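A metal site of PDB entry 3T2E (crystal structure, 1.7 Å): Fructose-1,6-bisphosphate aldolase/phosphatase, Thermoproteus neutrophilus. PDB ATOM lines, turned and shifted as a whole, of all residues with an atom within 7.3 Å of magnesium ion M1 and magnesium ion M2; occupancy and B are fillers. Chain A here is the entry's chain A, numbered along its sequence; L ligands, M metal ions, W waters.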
ATOM      1  N   LYS A   9      29.916  13.379   3.826  1.00  0.00           N
ATOM      2  CA  LYS A   9      29.254  14.392   4.705  1.00  0.00           C
ATOM      3  C   LYS A   9      30.291  15.207   5.404  1.00  0.00           C
ATOM      4  O   LYS A   9      31.352  14.636   5.746  1.00  0.00           O
ATOM      5  CB  LYS A   9      28.369  13.601   5.682  1.00  0.00           C
ATOM      6  CG  LYS A   9      27.696  14.477   6.817  1.00  0.00           C
ATOM      7  CD  LYS A   9      28.330  14.060   8.163  1.00  0.00           C
ATOM      8  CE  LYS A   9      29.289  14.980   8.657  1.00  0.00           C
ATOM      9  NZ  LYS A   9      29.829  14.755  10.092  1.00  0.00           N
ATOM     10  N   ALA A  10      30.065  16.503   5.598  1.00  0.00           N
ATOM     11  CA  ALA A  10      31.010  17.321   6.390  1.00  0.00           C
ATOM     12  C   ALA A  10      30.198  18.429   7.005  1.00  0.00           C
ATOM     13  O   ALA A  10      29.213  18.912   6.433  1.00  0.00           O
ATOM     14  CB  ALA A  10      32.068  17.968   5.461  1.00  0.00           C
ATOM     15  N   ASP A  11      30.771  18.912   8.086  1.00  0.00           N
ATOM     16  CA  ASP A  11      30.315  20.201   8.635  1.00  0.00           C
ATOM     17  C   ASP A  11      31.374  21.262   8.262  1.00  0.00           C
ATOM     18  O   ASP A  11      32.557  21.173   8.780  1.00  0.00           O
ATOM     19  CB  ASP A  11      30.245  20.041  10.142  1.00  0.00           C
ATOM     20  CG  ASP A  11      29.932  21.339  10.917  1.00  0.00           C
ATOM     21  OD1 ASP A  11      29.990  22.493  10.437  1.00  0.00           O
ATOM     22  OD2 ASP A  11      29.675  21.057  12.123  1.00  0.00           O
ATOM     23  N   VAL A  12      31.036  22.218   7.426  1.00  0.00           N
ATOM     24  CA  VAL A  12      31.975  23.241   7.020  1.00  0.00           C
ATOM     25  C   VAL A  12      31.489  24.577   7.475  1.00  0.00           C
ATOM     26  O   VAL A  12      31.873  25.577   6.920  1.00  0.00           O
ATOM     27  CB  VAL A  12      32.307  23.237   5.481  1.00  0.00           C
ATOM     28  CG1 VAL A  12      32.971  21.883   5.140  1.00  0.00           C
ATOM     29  CG2 VAL A  12      31.053  23.364   4.668  1.00  0.00           C
ATOM     30  N   GLY A  13      30.595  24.602   8.468  1.00  0.00           N
ATOM     31  CA  GLY A  13      30.181  25.943   8.992  1.00  0.00           C
ATOM     32  C   GLY A  13      28.706  25.905   9.371  1.00  0.00           C
ATOM     33  O   GLY A  13      27.904  25.420   8.657  1.00  0.00           O
ATOM     34  N   GLY A  14      28.424  26.458  10.522  1.00  0.00           N
ATOM     35  CA  GLY A  14      27.035  26.488  11.060  1.00  0.00           C
ATOM     36  C   GLY A  14      26.432  27.878  11.121  1.00  0.00           C
ATOM     37  O   GLY A  14      27.108  28.931  11.015  1.00  0.00           O
ATOM     38  N   GLY A  17      26.180  29.329  15.069  1.00  0.00           N
ATOM     39  CA  GLY A  17      26.802  28.311  15.952  1.00  0.00           C
ATOM     40  C   GLY A  17      26.808  26.966  15.252  1.00  0.00           C
ATOM     41  O   GLY A  17      27.196  26.858  14.051  1.00  0.00           O
ATOM     42  N   HIS A  18      26.354  25.935  15.975  1.00  0.00           N
ATOM     43  CA  HIS A  18      26.258  24.597  15.344  1.00  0.00           C
ATOM     44  C   HIS A  18      24.783  24.191  15.123  1.00  0.00           C
ATOM     45  O   HIS A  18      24.458  23.004  15.066  1.00  0.00           O
ATOM     46  CB  HIS A  18      26.924  23.592  16.229  1.00  0.00           C
ATOM     47  CG  HIS A  18      28.409  23.850  16.419  1.00  0.00           C
ATOM     48  ND1 HIS A  18      29.338  23.509  15.459  1.00  0.00           N
ATOM     49  CD2 HIS A  18      29.109  24.352  17.459  1.00  0.00           C
ATOM     50  CE1 HIS A  18      30.546  23.820  15.871  1.00  0.00           C
ATOM     51  NE2 HIS A  18      30.449  24.332  17.090  1.00  0.00           N
ATOM     52  N   ALA A  19      23.948  25.206  14.984  1.00  0.00           N
ATOM     53  CA  ALA A  19      22.488  24.886  15.024  1.00  0.00           C
ATOM     54  C   ALA A  19      21.923  24.427  13.706  1.00  0.00           C
ATOM     55  O   ALA A  19      20.876  23.742  13.664  1.00  0.00           O
ATOM     56  CB  ALA A  19      21.681  26.153  15.473  1.00  0.00           C
ATOM     57  N   HIS A  20      22.527  24.902  12.564  1.00  0.00           N
ATOM     58  CA  HIS A  20      21.896  24.617  11.272  1.00  0.00           C
ATOM     59  C   HIS A  20      22.935  24.974  10.201  1.00  0.00           C
ATOM     60  O   HIS A  20      24.050  25.329  10.568  1.00  0.00           O
ATOM     61  CB  HIS A  20      20.714  25.537  11.143  1.00  0.00           C
ATOM     62  CG  HIS A  20      19.591  25.028  10.276  1.00  0.00           C
ATOM     63  ND1 HIS A  20      19.154  23.697  10.186  1.00  0.00           N
ATOM     64  CD2 HIS A  20      18.699  25.748   9.555  1.00  0.00           C
ATOM     65  CE1 HIS A  20      18.085  23.633   9.376  1.00  0.00           C
ATOM     66  NE2 HIS A  20      17.790  24.869   9.009  1.00  0.00           N
ATOM     67  N   VAL A  50      21.338  17.754   8.102  1.00  0.00           N
ATOM     68  CA  VAL A  50      20.559  17.613   9.397  1.00  0.00           C
ATOM     69  C   VAL A  50      21.434  18.405  10.370  1.00  0.00           C
ATOM     70  O   VAL A  50      22.692  18.173  10.505  1.00  0.00           O
ATOM     71  CB  VAL A  50      20.512  16.125   9.806  1.00  0.00           C
ATOM     72  CG1 VAL A  50      19.998  15.945  11.283  1.00  0.00           C
ATOM     73  CG2 VAL A  50      19.529  15.309   8.875  1.00  0.00           C
ATOM     74  N   GLY A  51      20.829  19.431  11.013  1.00  0.00           N
ATOM     75  CA  GLY A  51      21.721  20.245  11.875  1.00  0.00           C
ATOM     76  C   GLY A  51      22.751  21.001  11.011  1.00  0.00           C
ATOM     77  O   GLY A  51      22.457  21.538   9.951  1.00  0.00           O
ATOM     78  N   ASP A  52      23.967  20.974  11.508  1.00  0.00           N
ATOM     79  CA  ASP A  52      25.051  21.704  10.819  1.00  0.00           C
ATOM     80  C   ASP A  52      25.871  20.762   9.940  1.00  0.00           C
ATOM     81  O   ASP A  52      26.983  21.159   9.488  1.00  0.00           O
ATOM     82  CB  ASP A  52      26.028  22.400  11.822  1.00  0.00           C
ATOM     83  CG  ASP A  52      26.652  21.396  12.805  1.00  0.00           C
ATOM     84  OD1 ASP A  52      26.415  20.144  12.792  1.00  0.00           O
ATOM     85  OD2 ASP A  52      27.491  21.823  13.696  1.00  0.00           O
ATOM     86  N   ASP A  53      25.337  19.591   9.615  1.00  0.00           N
ATOM     87  CA  ASP A  53      26.081  18.633   8.753  1.00  0.00           C
ATOM     88  C   ASP A  53      25.462  18.543   7.394  1.00  0.00           C
ATOM     89  O   ASP A  53      24.267  18.208   7.255  1.00  0.00           O
ATOM     90  CB  ASP A  53      26.095  17.248   9.394  1.00  0.00           C
ATOM     91  CG  ASP A  53      27.044  17.294  10.622  1.00  0.00           C
ATOM     92  OD1 ASP A  53      28.269  17.278  10.502  1.00  0.00           O
ATOM     93  OD2 ASP A  53      26.462  17.394  11.636  1.00  0.00           O
ATOM     94  N   ILE A  54      26.288  18.717   6.338  1.00  0.00           N
ATOM     95  CA  ILE A  54      25.787  18.603   4.958  1.00  0.00           C
ATOM     96  C   ILE A  54      26.204  17.231   4.384  1.00  0.00           C
ATOM     97  O   ILE A  54      27.368  16.936   4.395  1.00  0.00           O
ATOM     98  CB  ILE A  54      26.396  19.687   4.078  1.00  0.00           C
ATOM     99  CG1 ILE A  54      25.885  21.053   4.614  1.00  0.00           C
ATOM    100  CG2 ILE A  54      26.037  19.469   2.559  1.00  0.00           C
ATOM    101  CD1 ILE A  54      26.602  22.265   3.904  1.00  0.00           C
ATOM    102  N   TYR A  91      30.038  29.706  11.765  1.00  0.00           N
ATOM    103  CA  TYR A  91      30.728  29.210  12.895  1.00  0.00           C
ATOM    104  C   TYR A  91      31.303  27.823  12.628  1.00  0.00           C
ATOM    105  O   TYR A  91      30.639  26.898  12.178  1.00  0.00           O
ATOM    106  CB  TYR A  91      29.724  29.164  14.167  1.00  0.00           C
ATOM    107  CG  TYR A  91      30.539  29.018  15.415  1.00  0.00           C
ATOM    108  CD1 TYR A  91      31.227  30.109  15.955  1.00  0.00           C
ATOM    109  CD2 TYR A  91      30.701  27.754  16.035  1.00  0.00           C
ATOM    110  CE1 TYR A  91      32.089  29.985  17.039  1.00  0.00           C
ATOM    111  CE2 TYR A  91      31.584  27.583  17.154  1.00  0.00           C
ATOM    112  CZ  TYR A  91      32.257  28.743  17.637  1.00  0.00           C
ATOM    113  OH  TYR A  91      33.124  28.637  18.686  1.00  0.00           O
ATOM    114  N   GLY A  92      32.603  27.650  12.957  1.00  0.00           N
ATOM    115  CA  GLY A  92      33.314  26.416  12.548  1.00  0.00           C
ATOM    116  C   GLY A  92      33.547  26.382  11.016  1.00  0.00           C
ATOM    117  O   GLY A  92      33.563  25.326  10.399  1.00  0.00           O
ATOM    118  N   GLN A  95      35.396  23.668   9.406  1.00  0.00           N
ATOM    119  CA  GLN A  95      35.557  22.757  10.607  1.00  0.00           C
ATOM    120  C   GLN A  95      36.175  21.374  10.188  1.00  0.00           C
ATOM    121  O   GLN A  95      37.286  20.992  10.612  1.00  0.00           O
ATOM    122  CB  GLN A  95      34.160  22.622  11.387  1.00  0.00           C
ATOM    123  CG  GLN A  95      34.062  21.746  12.665  1.00  0.00           C
ATOM    124  CD  GLN A  95      32.950  22.146  13.714  1.00  0.00           C
ATOM    125  OE1 GLN A  95      31.778  22.579  13.411  1.00  0.00           O
ATOM    126  NE2 GLN A  95      33.341  21.980  14.991  1.00  0.00           N
ATOM    127  N   ASP A  96      35.477  20.652   9.318  1.00  0.00           N
ATOM    128  CA  ASP A  96      35.911  19.272   9.026  1.00  0.00           C
ATOM    129  C   ASP A  96      36.992  19.112   7.974  1.00  0.00           C
ATOM    130  O   ASP A  96      37.344  17.971   7.660  1.00  0.00           O
ATOM    131  CB  ASP A  96      34.703  18.389   8.644  1.00  0.00           C
ATOM    132  CG  ASP A  96      33.838  18.083   9.786  1.00  0.00           C
ATOM    133  OD1 ASP A  96      34.208  18.387  10.977  1.00  0.00           O
ATOM    134  OD2 ASP A  96      32.713  17.595   9.542  1.00  0.00           O
ATOM    135  N   ALA A 131      22.654  11.812  11.006  1.00  0.00           N
ATOM    136  CA  ALA A 131      22.354  12.244  12.408  1.00  0.00           C
ATOM    137  C   ALA A 131      23.268  13.378  12.782  1.00  0.00           C
ATOM    138  O   ALA A 131      24.381  13.442  12.282  1.00  0.00           O
ATOM    139  CB  ALA A 131      22.522  11.068  13.370  1.00  0.00           C
ATOM    140  N   ASP A 132      22.815  14.401  13.521  1.00  0.00           N
ATOM    141  CA  ASP A 132      23.724  15.423  13.995  1.00  0.00           C
ATOM    142  C   ASP A 132      23.796  15.304  15.541  1.00  0.00           C
ATOM    143  O   ASP A 132      22.879  14.781  16.234  1.00  0.00           O
ATOM    144  CB  ASP A 132      23.115  16.813  13.636  1.00  0.00           C
ATOM    145  CG  ASP A 132      24.089  17.982  13.944  1.00  0.00           C
ATOM    146  OD1 ASP A 132      25.317  17.706  14.109  1.00  0.00           O
ATOM    147  OD2 ASP A 132      23.591  19.101  14.059  1.00  0.00           O
ATOM    148  N   LYS A 133      24.927  15.789  16.045  1.00  0.00           N
ATOM    149  CA  LYS A 133      25.219  15.837  17.478  1.00  0.00           C
ATOM    150  C   LYS A 133      25.310  14.477  18.108  1.00  0.00           C
ATOM    151  O   LYS A 133      24.864  14.215  19.244  1.00  0.00           O
ATOM    152  CB  LYS A 133      24.143  16.722  18.240  1.00  0.00           C
ATOM    153  CG  LYS A 133      23.953  18.145  17.597  1.00  0.00           C
ATOM    154  CD  LYS A 133      25.223  18.977  17.880  1.00  0.00           C
ATOM    155  CE  LYS A 133      25.080  20.386  17.327  1.00  0.00           C
ATOM    156  NZ  LYS A 133      25.309  20.472  15.812  1.00  0.00           N
ATOM    157  N   THR A 134      25.955  13.536  17.378  1.00  0.00           N
ATOM    158  CA  THR A 134      26.215  12.247  17.985  1.00  0.00           C
ATOM    159  C   THR A 134      27.363  11.556  17.220  1.00  0.00           C
ATOM    160  O   THR A 134      27.957  12.185  16.373  1.00  0.00           O
ATOM    161  CB  THR A 134      24.887  11.399  18.050  1.00  0.00           C
ATOM    162  OG1 THR A 134      25.156  10.208  18.789  1.00  0.00           O
ATOM    163  CG2 THR A 134      24.369  11.014  16.663  1.00  0.00           C
ATOM    164  N   ASP A 233      32.889  12.016  14.527  1.00  0.00           N
ATOM    165  CA  ASP A 233      32.186  12.947  13.770  1.00  0.00           C
ATOM    166  C   ASP A 233      30.744  12.408  13.483  1.00  0.00           C
ATOM    167  O   ASP A 233      30.546  11.142  13.354  1.00  0.00           O
ATOM    168  CB  ASP A 233      32.953  13.219  12.451  1.00  0.00           C
ATOM    169  CG  ASP A 233      34.483  13.452  12.713  1.00  0.00           C
ATOM    170  OD1 ASP A 233      34.767  14.642  12.949  1.00  0.00           O
ATOM    171  OD2 ASP A 233      35.276  12.423  12.682  1.00  0.00           O
ATOM    172  N   ASP A 234      29.830  13.340  13.336  1.00  0.00           N
ATOM    173  CA  ASP A 234      28.357  12.999  13.228  1.00  0.00           C
ATOM    174  C   ASP A 234      28.193  12.077  11.990  1.00  0.00           C
ATOM    175  O   ASP A 234      28.780  12.376  10.901  1.00  0.00           O
ATOM    176  CB  ASP A 234      27.568  14.269  12.988  1.00  0.00           C
ATOM    177  CG  ASP A 234      27.718  15.311  14.117  1.00  0.00           C
ATOM    178  OD1 ASP A 234      27.863  14.845  15.253  1.00  0.00           O
ATOM    179  OD2 ASP A 234      27.787  16.529  13.899  1.00  0.00           O
ATOM    180  N   MET A 293      19.240  22.298  15.423  1.00  0.00           N
ATOM    181  CA  MET A 293      19.577  21.885  16.813  1.00  0.00           C
ATOM    182  C   MET A 293      19.394  23.125  17.687  1.00  0.00           C
ATOM    183  O   MET A 293      19.868  24.223  17.342  1.00  0.00           O
ATOM    184  CB  MET A 293      21.061  21.418  16.910  1.00  0.00           C
ATOM    185  CG  MET A 293      21.416  20.351  15.909  1.00  0.00           C
ATOM    186  SD  MET A 293      20.315  18.851  16.104  1.00  0.00           S
ATOM    187  CE  MET A 293      19.786  18.739  14.541  1.00  0.00           C
HETATM  188  C1  LIG L   1      29.096  19.525  19.659  1.00  0.00           C
HETATM  189  C2  LIG L   1      29.218  20.740  19.128  1.00  0.00           C
HETATM  190  C3  LIG L   1      28.725  21.912  19.928  1.00  0.00           C
HETATM  191  C4  LIG L   1      29.929  22.737  20.437  1.00  0.00           C
HETATM  192  C5  LIG L   1      29.511  23.885  21.359  1.00  0.00           C
HETATM  193  C6  LIG L   1      30.647  24.730  22.007  1.00  0.00           C
HETATM  194  O1  LIG L   1      29.593  18.555  18.805  1.00  0.00           O
HETATM  195  O2  LIG L   1      29.835  20.941  18.037  1.00  0.00           O
HETATM  196  O3  LIG L   1      27.874  21.381  21.011  1.00  0.00           O
HETATM  197  O4  LIG L   1      30.846  21.890  21.128  1.00  0.00           O
HETATM  198  O5  LIG L   1      28.569  24.705  20.663  1.00  0.00           O
HETATM  199  O6  LIG L   1      31.414  25.153  20.835  1.00  0.00           O
HETATM  200  P1  LIG L   1      32.574  26.239  21.225  1.00  0.00           P
HETATM  201  O7  LIG L   1      33.340  26.361  19.884  1.00  0.00           O
HETATM  202  O8  LIG L   1      33.439  25.603  22.269  1.00  0.00           O
HETATM  203  O9  LIG L   1      31.947  27.533  21.619  1.00  0.00           O
HETATM  204 MG    MG M   1      29.405  22.355  13.708  1.00  0.00          MG
HETATM  205 MG    MG M   2      27.188  18.340  13.443  1.00  0.00          MG
HETATM  206  O   HOH W   1      29.236  23.855  12.621  1.00  0.00           O
HETATM  207  O   HOH W   2      27.797  19.216  15.233  1.00  0.00           O
HETATM  208  O   HOH W   3      28.986  18.537  12.778  1.00  0.00           O
HETATM  209  O   HOH W   4      30.018  20.731  14.751  1.00  0.00           O
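Four residues have an atom within 4 Å of magnesium ion M1: Asp 11, His 18, Asp 52 and Gln 95.
The nearest printed residue that does not touch magnesium ion M1 is Tyr 91 (5.0 Å).
Magnesium ion M2 is bound by water W3 (1.9 Å), OD2 of Asp 234 (2.0 Å), OD1 of Asp 52 (2.1 Å), water W2 (2.1 Å), OD1 of Asp 132 (2.1 Å) and OD2 of Asp 53 (2.2 Å).
Magnesium ion M2 has six donor atoms within binding distance.
Lys 133 touches magnesium ion M2 (NZ to MG, 3.7 Å).
Along chain A the residues within 4 Å of magnesium ion M2 span positions 11 to 234.
The side-chain carboxylate (OD1) of Asp 234 sits at hydrogen-bond distance from the backbone NH (N) of Thr 134.
The side-chain carboxylate (OD1) of Asp 234 sits at hydrogen-bond distance from the backbone NH (N) of Lys 133, 3.2 Å away.
O of His 18 sits at hydrogen-bond distance from NZ of Lys 133 (2.8 Å).
OD1 of Asp 11 is in hydrogen-bond range of N of Gly 13 (2.9 Å).
The side-chain carboxylate of Asp 53 lies within salt-bridge range of the side-chain amino group of Lys 9, at 3.0 Å.
The side-chain carboxylate (OD2) of Asp 132 lies within salt-bridge range of the side-chain amino group (NZ) of Lys 133, at 2.8 Å.
The side-chain amino group (NZ) of Lys 9 sits at hydrogen-bond distance from the backbone carbonyl oxygen (O) of Asp 234, at 2.7 Å.
The side-chain carboxylate (OD1) of Asp 52 lies close to the side-chain amino group (NZ) of Lys 133 (3.2 Å).
O7 of the ligand sits at hydrogen-bond distance from OH of Tyr 91 (2.6 Å).
Water W1 lies within hydrogen-bond range of the side-chain carboxylate (OD1) of Asp 11, the backbone carbonyl oxygen (O) of Tyr 91 and the backbone NH (N) of Gly 14.
Water W1 is bound to magnesium ion M1, at 1.9 Å.
Magnesium ion M1 is bound by OD2 of Asp 52 (2.0 Å).
Water W4 is bound to magnesium ion M1, 2.0 Å away.
The side-chain carboxylate (OD2) of Asp 11 binds magnesium ion M1 (2.1 Å).
ND1 of His 18 is bound to magnesium ion M1 (2.1 Å).
OE1 of Gln 95 is bound to magnesium ion M1, at 2.4 Å.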
